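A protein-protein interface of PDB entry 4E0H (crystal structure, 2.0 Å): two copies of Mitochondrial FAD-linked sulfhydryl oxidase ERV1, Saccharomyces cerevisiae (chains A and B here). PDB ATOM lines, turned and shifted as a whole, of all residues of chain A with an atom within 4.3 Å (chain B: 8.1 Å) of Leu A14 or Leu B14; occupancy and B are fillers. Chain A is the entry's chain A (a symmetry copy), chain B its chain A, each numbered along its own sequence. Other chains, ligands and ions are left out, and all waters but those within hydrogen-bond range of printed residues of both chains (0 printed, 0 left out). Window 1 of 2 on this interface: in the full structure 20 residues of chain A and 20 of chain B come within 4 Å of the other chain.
Leu A7 touches Ser B17, and with the chains exchanged Ser A17 touches Leu B7. Ser B10 touches its own counterpart, Ser A10. Leu B14 touches its own counterpart, Leu A14. Leu A14 touches Phe B41, and with the chains exchanged Phe A41 touches Leu B14. Of the 13 pairs that touch across the chains among the printed residues, 10 have their exchanged pair printed and touching as well.
OG of Ser B10 is in hydrogen-bond range of O of Gln B6 (2.7 Å). The backbone carbonyl oxygen (O) of Leu B7 sits at hydrogen-bond distance from the side-chain hydroxyl (OG) of Ser B11. The side-chain hydroxyl (OG1) of Thr B13 sits at hydrogen-bond distance from the backbone carbonyl oxygen (O) of Arg B9. O of Thr B13 lies within hydrogen-bond range of OG of Ser B17 (2.7 Å). The backbone carbonyl oxygen (O) of Leu A7 sits at hydrogen-bond distance from the side-chain hydroxyl (OG) of Ser A11, 2.8 Å away. The backbone carbonyl oxygen of Thr A13 sits at hydrogen-bond distance from the side-chain hydroxyl of Ser A17 (2.7 Å).
Among the printed residues, pairs that only touch across the chains: Leu A7 with Ser B17, Ser A10 with Ser B10, Ser A10 with Thr B13, Ser A11 with Leu B14, Thr A13 with Ser B10, Leu A14 with Ser B11, Leu A14 with Leu B14, Leu A14 with Phe B41, Ser A17 with Leu B7, Ser A17 with Pro B46, Val A18 with Ile B44, Val A18 with Pro B46 and Phe A41 with Leu B14.
Printed residues of chain B within 4 Å of Thr A13: Ser B10. Leu A14 touches three residues of chain B. Printed residues of chain B within 4 Å of Ser A17: Leu B7 and Pro B46. Printed residues of chain B within 4 Å of Val A18: Ile B44 and Pro B46. Printed residues of chain A within 4 Å of Thr B13: Ser A10. Leu B14 touches just these residues of chain A: Ser A11, Leu A14 and Phe A41. Printed residues of chain A within 4 Å of Ile B44: Val A18 (3.7 Å). The nearest printed residue of chain A that does not touch Leu B14 is Leu A7 (4.2 Å). The nearest printed residue of chain B that does not touch Thr A13 is Leu B7 (4.4 Å).
Hydrophobic or aromatic side chains of chain A within 4 Å of the printed part of chain B: Leu A7, Leu A14, Val A18 and Phe A41. Among the printed residues, 13 pairs touch across the chains. Among the printed residues, no Asp or Glu carboxylate lies within 4 Å of a Lys or Arg side-chain nitrogen of the other chain.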
ATOM      1  N   LEU A   7     -22.663  17.083 -10.522  1.00  0.00           N
ATOM      2  CA  LEU A   7     -21.477  17.916 -10.671  1.00  0.00           C
ATOM      3  C   LEU A   7     -21.540  19.085  -9.691  1.00  0.00           C
ATOM      4  O   LEU A   7     -20.543  19.442  -9.085  1.00  0.00           O
ATOM      5  CB  LEU A   7     -21.366  18.456 -12.092  1.00  0.00           C
ATOM      6  CG  LEU A   7     -20.214  19.440 -12.315  1.00  0.00           C
ATOM      7  CD1 LEU A   7     -18.875  18.723 -12.121  1.00  0.00           C
ATOM      8  CD2 LEU A   7     -20.323  20.099 -13.720  1.00  0.00           C
ATOM      9  N   SER A  10     -21.087  17.954  -6.044  1.00  0.00           N
ATOM     10  CA  SER A  10     -19.687  17.520  -5.867  1.00  0.00           C
ATOM     11  C   SER A  10     -18.795  18.754  -5.750  1.00  0.00           C
ATOM     12  O   SER A  10     -17.844  18.816  -4.955  1.00  0.00           O
ATOM     13  CB  SER A  10     -19.234  16.683  -7.063  1.00  0.00           C
ATOM     14  OG  SER A  10     -19.999  15.494  -7.143  1.00  0.00           O
ATOM     15  N   SER A  11     -19.081  19.728  -6.590  1.00  0.00           N
ATOM     16  CA  SER A  11     -18.178  20.883  -6.683  1.00  0.00           C
ATOM     17  C   SER A  11     -18.332  21.807  -5.461  1.00  0.00           C
ATOM     18  O   SER A  11     -17.346  22.283  -4.947  1.00  0.00           O
ATOM     19  CB  SER A  11     -18.344  21.649  -8.021  1.00  0.00           C
ATOM     20  OG  SER A  11     -18.089  20.793  -9.128  1.00  0.00           O
ATOM     21  N   TRP A  12     -19.556  21.987  -4.957  1.00  0.00           N
ATOM     22  CA  TRP A  12     -19.723  22.731  -3.690  1.00  0.00           C
ATOM     23  C   TRP A  12     -19.057  21.984  -2.522  1.00  0.00           C
ATOM     24  O   TRP A  12     -18.464  22.618  -1.668  1.00  0.00           O
ATOM     25  CB  TRP A  12     -21.195  22.975  -3.354  1.00  0.00           C
ATOM     26  CG  TRP A  12     -21.879  23.959  -4.316  1.00  0.00           C
ATOM     27  CD1 TRP A  12     -22.919  23.709  -5.099  1.00  0.00           C
ATOM     28  CD2 TRP A  12     -21.537  25.339  -4.528  1.00  0.00           C
ATOM     29  NE1 TRP A  12     -23.260  24.836  -5.836  1.00  0.00           N
ATOM     30  CE2 TRP A  12     -22.448  25.857  -5.458  1.00  0.00           C
ATOM     31  CE3 TRP A  12     -20.563  26.177  -4.013  1.00  0.00           C
ATOM     32  CZ2 TRP A  12     -22.398  27.151  -5.898  1.00  0.00           C
ATOM     33  CZ3 TRP A  12     -20.525  27.493  -4.461  1.00  0.00           C
ATOM     34  CH2 TRP A  12     -21.413  27.944  -5.418  1.00  0.00           C
ATOM     35  N   THR A  13     -19.181  20.658  -2.471  1.00  0.00           N
ATOM     36  CA  THR A  13     -18.474  19.864  -1.449  1.00  0.00           C
ATOM     37  C   THR A  13     -16.982  20.190  -1.457  1.00  0.00           C
ATOM     38  O   THR A  13     -16.407  20.472  -0.410  1.00  0.00           O
ATOM     39  CB  THR A  13     -18.702  18.347  -1.625  1.00  0.00           C
ATOM     40  OG1 THR A  13     -20.076  18.064  -1.405  1.00  0.00           O
ATOM     41  CG2 THR A  13     -17.881  17.516  -0.601  1.00  0.00           C
ATOM     42  N   LEU A  14     -16.368  20.193  -2.642  1.00  0.00           N
ATOM     43  CA  LEU A  14     -14.954  20.529  -2.766  1.00  0.00           C
ATOM     44  C   LEU A  14     -14.660  21.963  -2.345  1.00  0.00           C
ATOM     45  O   LEU A  14     -13.712  22.194  -1.604  1.00  0.00           O
ATOM     46  CB  LEU A  14     -14.460  20.346  -4.212  1.00  0.00           C
ATOM     47  CG  LEU A  14     -12.976  20.805  -4.333  1.00  0.00           C
ATOM     48  CD1 LEU A  14     -12.015  19.899  -3.464  1.00  0.00           C
ATOM     49  CD2 LEU A  14     -12.454  20.825  -5.740  1.00  0.00           C
ATOM     50  N   LEU A  15     -15.422  22.951  -2.834  1.00  0.00           N
ATOM     51  CA  LEU A  15     -15.154  24.361  -2.471  1.00  0.00           C
ATOM     52  C   LEU A  15     -15.258  24.708  -1.002  1.00  0.00           C
ATOM     53  O   LEU A  15     -14.377  25.382  -0.451  1.00  0.00           O
ATOM     54  CB  LEU A  15     -16.126  25.288  -3.234  1.00  0.00           C
ATOM     55  CG  LEU A  15     -15.926  25.296  -4.767  1.00  0.00           C
ATOM     56  CD1 LEU A  15     -17.021  26.060  -5.517  1.00  0.00           C
ATOM     57  CD2 LEU A  15     -14.591  25.997  -4.991  1.00  0.00           C
ATOM     58  N   HIS A  16     -16.353  24.291  -0.370  1.00  0.00           N
ATOM     59  CA  HIS A  16     -16.582  24.482   1.091  1.00  0.00           C
ATOM     60  C   HIS A  16     -15.562  23.708   1.941  1.00  0.00           C
ATOM     61  O   HIS A  16     -15.161  24.199   2.974  1.00  0.00           O
ATOM     62  CB  HIS A  16     -17.997  24.074   1.507  1.00  0.00           C
ATOM     63  CG  HIS A  16     -19.074  24.976   0.960  1.00  0.00           C
ATOM     64  ND1 HIS A  16     -19.090  26.325   1.202  1.00  0.00           N
ATOM     65  CD2 HIS A  16     -20.155  24.723   0.179  1.00  0.00           C
ATOM     66  CE1 HIS A  16     -20.120  26.878   0.586  1.00  0.00           C
ATOM     67  NE2 HIS A  16     -20.780  25.929  -0.051  1.00  0.00           N
ATOM     68  N   SER A  17     -15.171  22.505   1.504  1.00  0.00           N
ATOM     69  CA  SER A  17     -14.077  21.738   2.150  1.00  0.00           C
ATOM     70  C   SER A  17     -12.749  22.404   2.073  1.00  0.00           C
ATOM     71  O   SER A  17     -12.004  22.380   3.027  1.00  0.00           O
ATOM     72  CB  SER A  17     -13.999  20.308   1.652  1.00  0.00           C
ATOM     73  OG  SER A  17     -15.245  19.682   1.952  1.00  0.00           O
ATOM     74  N   VAL A  18     -12.408  22.998   0.941  1.00  0.00           N
ATOM     75  CA  VAL A  18     -11.187  23.761   0.857  1.00  0.00           C
ATOM     76  C   VAL A  18     -11.225  24.979   1.767  1.00  0.00           C
ATOM     77  O   VAL A  18     -10.210  25.301   2.402  1.00  0.00           O
ATOM     78  CB  VAL A  18     -10.944  24.201  -0.581  1.00  0.00           C
ATOM     79  CG1 VAL A  18      -9.917  25.298  -0.609  1.00  0.00           C
ATOM     80  CG2 VAL A  18     -10.441  23.007  -1.374  1.00  0.00           C
ATOM     81  N   PHE A  41     -11.166  28.157 -11.480  1.00  0.00           N
ATOM     82  CA  PHE A  41     -12.364  27.315 -11.319  1.00  0.00           C
ATOM     83  C   PHE A  41     -13.529  27.907 -12.116  1.00  0.00           C
ATOM     84  O   PHE A  41     -14.245  27.203 -12.841  1.00  0.00           O
ATOM     85  CB  PHE A  41     -12.732  27.222  -9.832  1.00  0.00           C
ATOM     86  CG  PHE A  41     -13.966  26.389  -9.575  1.00  0.00           C
ATOM     87  CD1 PHE A  41     -13.873  25.027  -9.375  1.00  0.00           C
ATOM     88  CD2 PHE A  41     -15.215  26.980  -9.525  1.00  0.00           C
ATOM     89  CE1 PHE A  41     -15.044  24.262  -9.157  1.00  0.00           C
ATOM     90  CE2 PHE A  41     -16.379  26.212  -9.308  1.00  0.00           C
ATOM     91  CZ  PHE A  41     -16.281  24.873  -9.134  1.00  0.00           C
ATOM     92  N   TYR A  45     -15.214  25.596 -15.023  1.00  0.00           N
ATOM     93  CA  TYR A  45     -16.332  24.822 -14.489  1.00  0.00           C
ATOM     94  C   TYR A  45     -17.201  24.318 -15.632  1.00  0.00           C
ATOM     95  O   TYR A  45     -17.716  25.113 -16.441  1.00  0.00           O
ATOM     96  CB  TYR A  45     -17.169  25.633 -13.526  1.00  0.00           C
ATOM     97  CG  TYR A  45     -18.203  24.790 -12.837  1.00  0.00           C
ATOM     98  CD1 TYR A  45     -17.831  23.776 -11.944  1.00  0.00           C
ATOM     99  CD2 TYR A  45     -19.565  24.993 -13.075  1.00  0.00           C
ATOM    100  CE1 TYR A  45     -18.802  22.998 -11.300  1.00  0.00           C
ATOM    101  CE2 TYR A  45     -20.530  24.214 -12.444  1.00  0.00           C
ATOM    102  CZ  TYR A  45     -20.134  23.244 -11.558  1.00  0.00           C
ATOM    103  OH  TYR A  45     -21.099  22.502 -10.940  1.00  0.00           O
ATOM    104  N   GLN B   6     -16.430  10.866   0.634  1.00  0.00           N
ATOM    105  CA  GLN B   6     -17.346  11.770  -0.072  1.00  0.00           C
ATOM    106  C   GLN B   6     -16.606  12.890  -0.728  1.00  0.00           C
ATOM    107  O   GLN B   6     -16.899  13.263  -1.885  1.00  0.00           O
ATOM    108  CB  GLN B   6     -18.391  12.360   0.862  1.00  0.00           C
ATOM    109  CG  GLN B   6     -19.658  12.718   0.088  1.00  0.00           C
ATOM    110  CD  GLN B   6     -20.510  11.496  -0.101  1.00  0.00           C
ATOM    111  OE1 GLN B   6     -21.060  10.962   0.883  1.00  0.00           O
ATOM    112  NE2 GLN B   6     -20.613  11.010  -1.337  1.00  0.00           N
ATOM    113  N   LEU B   7     -15.638  13.435  -0.006  1.00  0.00           N
ATOM    114  CA  LEU B   7     -14.774  14.457  -0.584  1.00  0.00           C
ATOM    115  C   LEU B   7     -14.045  13.890  -1.800  1.00  0.00           C
ATOM    116  O   LEU B   7     -13.905  14.562  -2.809  1.00  0.00           O
ATOM    117  CB  LEU B   7     -13.750  14.943   0.434  1.00  0.00           C
ATOM    118  CG  LEU B   7     -12.720  15.933  -0.115  1.00  0.00           C
ATOM    119  CD1 LEU B   7     -13.419  17.229  -0.536  1.00  0.00           C
ATOM    120  CD2 LEU B   7     -11.597  16.191   0.931  1.00  0.00           C
ATOM    121  N   GLY B   8     -13.543  12.653  -1.685  1.00  0.00           N
ATOM    122  CA  GLY B   8     -12.800  11.997  -2.795  1.00  0.00           C
ATOM    123  C   GLY B   8     -13.679  11.763  -4.009  1.00  0.00           C
ATOM    124  O   GLY B   8     -13.319  12.185  -5.095  1.00  0.00           O
ATOM    125  N   ARG B   9     -14.834  11.119  -3.856  1.00  0.00           N
ATOM    126  CA  ARG B   9     -15.745  10.941  -4.988  1.00  0.00           C
ATOM    127  C   ARG B   9     -16.134  12.273  -5.599  1.00  0.00           C
ATOM    128  O   ARG B   9     -16.163  12.377  -6.830  1.00  0.00           O
ATOM    129  CB  ARG B   9     -17.070  10.327  -4.583  1.00  0.00           C
ATOM    130  CG  ARG B   9     -17.057   8.941  -4.384  1.00  0.00           C
ATOM    131  CD  ARG B   9     -18.466   8.405  -4.141  1.00  0.00           C
ATOM    132  NE  ARG B   9     -18.838   8.729  -2.779  1.00  0.00           N
ATOM    133  CZ  ARG B   9     -18.537   8.002  -1.689  1.00  0.00           C
ATOM    134  NH1 ARG B   9     -17.857   6.863  -1.757  1.00  0.00           N
ATOM    135  NH2 ARG B   9     -18.926   8.436  -0.499  1.00  0.00           N
ATOM    136  N   SER B  10     -16.415  13.288  -4.768  1.00  0.00           N
ATOM    137  CA  SER B  10     -16.842  14.601  -5.289  1.00  0.00           C
ATOM    138  C   SER B  10     -15.710  15.198  -6.123  1.00  0.00           C
ATOM    139  O   SER B  10     -15.915  15.811  -7.183  1.00  0.00           O
ATOM    140  CB  SER B  10     -17.172  15.549  -4.137  1.00  0.00           C
ATOM    141  OG  SER B  10     -18.272  15.052  -3.397  1.00  0.00           O
ATOM    142  N   SER B  11     -14.506  15.055  -5.609  1.00  0.00           N
ATOM    143  CA  SER B  11     -13.371  15.743  -6.239  1.00  0.00           C
ATOM    144  C   SER B  11     -12.961  15.050  -7.551  1.00  0.00           C
ATOM    145  O   SER B  11     -12.677  15.723  -8.515  1.00  0.00           O
ATOM    146  CB  SER B  11     -12.175  15.908  -5.264  1.00  0.00           C
ATOM    147  OG  SER B  11     -12.561  16.646  -4.111  1.00  0.00           O
ATOM    148  N   TRP B  12     -13.012  13.717  -7.603  1.00  0.00           N
ATOM    149  CA  TRP B  12     -12.787  13.026  -8.890  1.00  0.00           C
ATOM    150  C   TRP B  12     -13.889  13.379  -9.904  1.00  0.00           C
ATOM    151  O   TRP B  12     -13.592  13.549 -11.073  1.00  0.00           O
ATOM    152  CB  TRP B  12     -12.725  11.507  -8.727  1.00  0.00           C
ATOM    153  CG  TRP B  12     -11.478  11.032  -7.964  1.00  0.00           C
ATOM    154  CD1 TRP B  12     -11.455  10.361  -6.821  1.00  0.00           C
ATOM    155  CD2 TRP B  12     -10.106  11.202  -8.359  1.00  0.00           C
ATOM    156  NE1 TRP B  12     -10.148  10.109  -6.426  1.00  0.00           N
ATOM    157  CE2 TRP B  12      -9.311  10.578  -7.388  1.00  0.00           C
ATOM    158  CE3 TRP B  12      -9.486  11.805  -9.439  1.00  0.00           C
ATOM    159  CZ2 TRP B  12      -7.945  10.565  -7.450  1.00  0.00           C
ATOM    160  CZ3 TRP B  12      -8.097  11.781  -9.497  1.00  0.00           C
ATOM    161  CH2 TRP B  12      -7.354  11.199  -8.489  1.00  0.00           C
ATOM    162  N   THR B  13     -15.145  13.456  -9.467  1.00  0.00           N
ATOM    163  CA  THR B  13     -16.236  13.903 -10.352  1.00  0.00           C
ATOM    164  C   THR B  13     -15.886  15.243 -10.996  1.00  0.00           C
ATOM    165  O   THR B  13     -15.989  15.388 -12.210  1.00  0.00           O
ATOM    166  CB  THR B  13     -17.591  13.989  -9.616  1.00  0.00           C
ATOM    167  OG1 THR B  13     -17.974  12.682  -9.213  1.00  0.00           O
ATOM    168  CG2 THR B  13     -18.713  14.547 -10.533  1.00  0.00           C
ATOM    169  N   LEU B  14     -15.434  16.204 -10.189  1.00  0.00           N
ATOM    170  CA  LEU B  14     -15.035  17.508 -10.708  1.00  0.00           C
ATOM    171  C   LEU B  14     -13.845  17.416 -11.654  1.00  0.00           C
ATOM    172  O   LEU B  14     -13.873  18.017 -12.722  1.00  0.00           O
ATOM    173  CB  LEU B  14     -14.664  18.474  -9.568  1.00  0.00           C
ATOM    174  CG  LEU B  14     -14.150  19.822 -10.155  1.00  0.00           C
ATOM    175  CD1 LEU B  14     -15.282  20.573 -10.963  1.00  0.00           C
ATOM    176  CD2 LEU B  14     -13.603  20.769  -9.127  1.00  0.00           C
ATOM    177  N   LEU B  15     -12.769  16.712 -11.276  1.00  0.00           N
ATOM    178  CA  LEU B  15     -11.582  16.619 -12.155  1.00  0.00           C
ATOM    179  C   LEU B  15     -11.797  15.982 -13.511  1.00  0.00           C
ATOM    180  O   LEU B  15     -11.346  16.514 -14.534  1.00  0.00           O
ATOM    181  CB  LEU B  15     -10.469  15.819 -11.442  1.00  0.00           C
ATOM    182  CG  LEU B  15      -9.897  16.509 -10.183  1.00  0.00           C
ATOM    183  CD1 LEU B  15      -8.944  15.617  -9.383  1.00  0.00           C
ATOM    184  CD2 LEU B  15      -9.124  17.715 -10.705  1.00  0.00           C
ATOM    185  N   HIS B  16     -12.448  14.821 -13.525  1.00  0.00           N
ATOM    186  CA  HIS B  16     -12.809  14.096 -14.776  1.00  0.00           C
ATOM    187  C   HIS B  16     -13.809  14.888 -15.633  1.00  0.00           C
ATOM    188  O   HIS B  16     -13.718  14.843 -16.841  1.00  0.00           O
ATOM    189  CB  HIS B  16     -13.382  12.706 -14.488  1.00  0.00           C
ATOM    190  CG  HIS B  16     -12.374  11.741 -13.917  1.00  0.00           C
ATOM    191  ND1 HIS B  16     -11.207  11.433 -14.567  1.00  0.00           N
ATOM    192  CD2 HIS B  16     -12.356  11.033 -12.759  1.00  0.00           C
ATOM    193  CE1 HIS B  16     -10.497  10.591 -13.837  1.00  0.00           C
ATOM    194  NE2 HIS B  16     -11.167  10.337 -12.729  1.00  0.00           N
ATOM    195  N   SER B  17     -14.759  15.585 -14.999  1.00  0.00           N
ATOM    196  CA  SER B  17     -15.676  16.512 -15.707  1.00  0.00           C
ATOM    197  C   SER B  17     -14.990  17.669 -16.344  1.00  0.00           C
ATOM    198  O   SER B  17     -15.339  18.051 -17.438  1.00  0.00           O
ATOM    199  CB  SER B  17     -16.824  16.975 -14.830  1.00  0.00           C
ATOM    200  OG  SER B  17     -17.552  15.816 -14.431  1.00  0.00           O
ATOM    201  N   VAL B  18     -14.015  18.265 -15.678  1.00  0.00           N
ATOM    202  CA  VAL B  18     -13.239  19.308 -16.301  1.00  0.00           C
ATOM    203  C   VAL B  18     -12.438  18.781 -17.482  1.00  0.00           C
ATOM    204  O   VAL B  18     -12.340  19.465 -18.512  1.00  0.00           O
ATOM    205  CB  VAL B  18     -12.297  19.940 -15.283  1.00  0.00           C
ATOM    206  CG1 VAL B  18     -11.237  20.731 -15.995  1.00  0.00           C
ATOM    207  CG2 VAL B  18     -13.105  20.858 -14.382  1.00  0.00           C
ATOM    208  N   ALA B  19     -11.821  17.591 -17.365  1.00  0.00           N
ATOM    209  CA  ALA B  19     -11.093  17.057 -18.502  1.00  0.00           C
ATOM    210  C   ALA B  19     -12.063  16.712 -19.648  1.00  0.00           C
ATOM    211  O   ALA B  19     -11.738  16.946 -20.796  1.00  0.00           O
ATOM    212  CB  ALA B  19     -10.223  15.784 -18.082  1.00  0.00           C
ATOM    213  N   ALA B  20     -13.261  16.207 -19.357  1.00  0.00           N
ATOM    214  CA  ALA B  20     -14.242  15.866 -20.438  1.00  0.00           C
ATOM    215  C   ALA B  20     -14.742  17.067 -21.219  1.00  0.00           C
ATOM    216  O   ALA B  20     -15.223  16.913 -22.350  1.00  0.00           O
ATOM    217  CB  ALA B  20     -15.482  15.136 -19.861  1.00  0.00           C
ATOM    218  N   SER B  21     -14.673  18.240 -20.606  1.00  0.00           N
ATOM    219  CA  SER B  21     -15.139  19.476 -21.194  1.00  0.00           C
ATOM    220  C   SER B  21     -14.016  20.214 -21.878  1.00  0.00           C
ATOM    221  O   SER B  21     -14.239  21.236 -22.495  1.00  0.00           O
ATOM    222  CB  SER B  21     -15.672  20.380 -20.102  1.00  0.00           C
ATOM    223  OG  SER B  21     -17.027  20.043 -19.938  1.00  0.00           O
ATOM    224  N   PHE B  37      -4.265  25.034 -12.457  1.00  0.00           N
ATOM    225  CA  PHE B  37      -5.379  24.555 -11.687  1.00  0.00           C
ATOM    226  C   PHE B  37      -4.965  23.310 -10.932  1.00  0.00           C
ATOM    227  O   PHE B  37      -5.187  23.143  -9.721  1.00  0.00           O
ATOM    228  CB  PHE B  37      -6.510  24.178 -12.614  1.00  0.00           C
ATOM    229  CG  PHE B  37      -7.739  23.689 -11.880  1.00  0.00           C
ATOM    230  CD1 PHE B  37      -8.493  24.576 -11.113  1.00  0.00           C
ATOM    231  CD2 PHE B  37      -8.134  22.352 -11.969  1.00  0.00           C
ATOM    232  CE1 PHE B  37      -9.635  24.134 -10.435  1.00  0.00           C
ATOM    233  CE2 PHE B  37      -9.290  21.902 -11.310  1.00  0.00           C
ATOM    234  CZ  PHE B  37     -10.022  22.789 -10.543  1.00  0.00           C
ATOM    235  N   PHE B  41      -4.649  22.702  -7.015  1.00  0.00           N
ATOM    236  CA  PHE B  41      -5.526  21.666  -6.441  1.00  0.00           C
ATOM    237  C   PHE B  41      -4.718  20.751  -5.518  1.00  0.00           C
ATOM    238  O   PHE B  41      -5.130  20.435  -4.393  1.00  0.00           O
ATOM    239  CB  PHE B  41      -6.165  20.848  -7.571  1.00  0.00           C
ATOM    240  CG  PHE B  41      -7.070  19.746  -7.071  1.00  0.00           C
ATOM    241  CD1 PHE B  41      -8.408  19.982  -6.830  1.00  0.00           C
ATOM    242  CD2 PHE B  41      -6.574  18.474  -6.853  1.00  0.00           C
ATOM    243  CE1 PHE B  41      -9.233  18.942  -6.340  1.00  0.00           C
ATOM    244  CE2 PHE B  41      -7.402  17.441  -6.365  1.00  0.00           C
ATOM    245  CZ  PHE B  41      -8.709  17.686  -6.111  1.00  0.00           C
ATOM    246  N   ILE B  44      -3.899  22.426  -2.099  1.00  0.00           N
ATOM    247  CA  ILE B  44      -5.002  22.768  -1.198  1.00  0.00           C
ATOM    248  C   ILE B  44      -6.007  21.655  -0.949  1.00  0.00           C
ATOM    249  O   ILE B  44      -6.918  21.851  -0.170  1.00  0.00           O
ATOM    250  CB  ILE B  44      -5.751  24.020  -1.708  1.00  0.00           C
ATOM    251  CG1 ILE B  44      -6.590  23.740  -2.947  1.00  0.00           C
ATOM    252  CG2 ILE B  44      -4.797  25.172  -1.968  1.00  0.00           C
ATOM    253  CD1 ILE B  44      -7.472  24.980  -3.303  1.00  0.00           C
ATOM    254  N   TYR B  45      -5.858  20.507  -1.610  1.00  0.00           N
ATOM    255  CA  TYR B  45      -6.805  19.412  -1.412  1.00  0.00           C
ATOM    256  C   TYR B  45      -6.883  19.060   0.066  1.00  0.00           C
ATOM    257  O   TYR B  45      -5.863  18.722   0.697  1.00  0.00           O
ATOM    258  CB  TYR B  45      -6.426  18.187  -2.213  1.00  0.00           C
ATOM    259  CG  TYR B  45      -7.492  17.131  -2.157  1.00  0.00           C
ATOM    260  CD1 TYR B  45      -8.751  17.343  -2.737  1.00  0.00           C
ATOM    261  CD2 TYR B  45      -7.256  15.910  -1.521  1.00  0.00           C
ATOM    262  CE1 TYR B  45      -9.737  16.350  -2.687  1.00  0.00           C
ATOM    263  CE2 TYR B  45      -8.239  14.927  -1.462  1.00  0.00           C
ATOM    264  CZ  TYR B  45      -9.453  15.157  -2.058  1.00  0.00           C
ATOM    265  OH  TYR B  45     -10.397  14.173  -2.000  1.00  0.00           O
ATOM    266  N   PRO B  46      -8.080  19.144   0.650  1.00  0.00           N
ATOM    267  CA  PRO B  46      -8.166  19.053   2.103  1.00  0.00           C
ATOM    268  C   PRO B  46      -8.118  17.667   2.686  1.00  0.00           C
ATOM    269  O   PRO B  46      -9.019  17.324   3.447  1.00  0.00           O
ATOM    270  CB  PRO B  46      -9.548  19.627   2.392  1.00  0.00           C
ATOM    271  CG  PRO B  46     -10.318  19.404   1.209  1.00  0.00           C
ATOM    272  CD  PRO B  46      -9.374  19.485   0.036  1.00  0.00           C
ATOM    273  N   MET B  75      -5.645  12.011 -16.364  1.00  0.00           N
ATOM    274  CA  MET B  75      -6.511  11.960 -15.183  1.00  0.00           C
ATOM    275  C   MET B  75      -6.894  10.534 -14.817  1.00  0.00           C
ATOM    276  O   MET B  75      -6.927  10.167 -13.636  1.00  0.00           O
ATOM    277  CB  MET B  75      -7.806  12.751 -15.510  1.00  0.00           C
ATOM    278  CG  MET B  75      -8.449  13.436 -14.273  1.00  0.00           C
ATOM    279  SD  MET B  75      -7.351  14.637 -13.450  1.00  0.00           S
ATOM    280  CE  MET B  75      -7.434  15.935 -14.652  1.00  0.00           C
ATOM    281  N   TRP B 100     -17.162   9.610 -18.736  1.00  0.00           N
ATOM    282  CA  TRP B 100     -17.109  10.990 -18.244  1.00  0.00           C
ATOM    283  C   TRP B 100     -17.499  12.003 -19.281  1.00  0.00           C
ATOM    284  O   TRP B 100     -18.070  13.038 -18.961  1.00  0.00           O
ATOM    285  CB  TRP B 100     -15.707  11.314 -17.692  1.00  0.00           C
ATOM    286  CG  TRP B 100     -15.479  10.640 -16.407  1.00  0.00           C
ATOM    287  CD1 TRP B 100     -14.657   9.561 -16.163  1.00  0.00           C
ATOM    288  CD2 TRP B 100     -16.151  10.913 -15.179  1.00  0.00           C
ATOM    289  NE1 TRP B 100     -14.756   9.187 -14.838  1.00  0.00           N
ATOM    290  CE2 TRP B 100     -15.672   9.996 -14.220  1.00  0.00           C
ATOM    291  CE3 TRP B 100     -17.081  11.882 -14.786  1.00  0.00           C
ATOM    292  CZ2 TRP B 100     -16.104  10.008 -12.894  1.00  0.00           C
ATOM    293  CZ3 TRP B 100     -17.509  11.900 -13.465  1.00  0.00           C
ATOM    294  CH2 TRP B 100     -17.019  10.968 -12.538  1.00  0.00           C
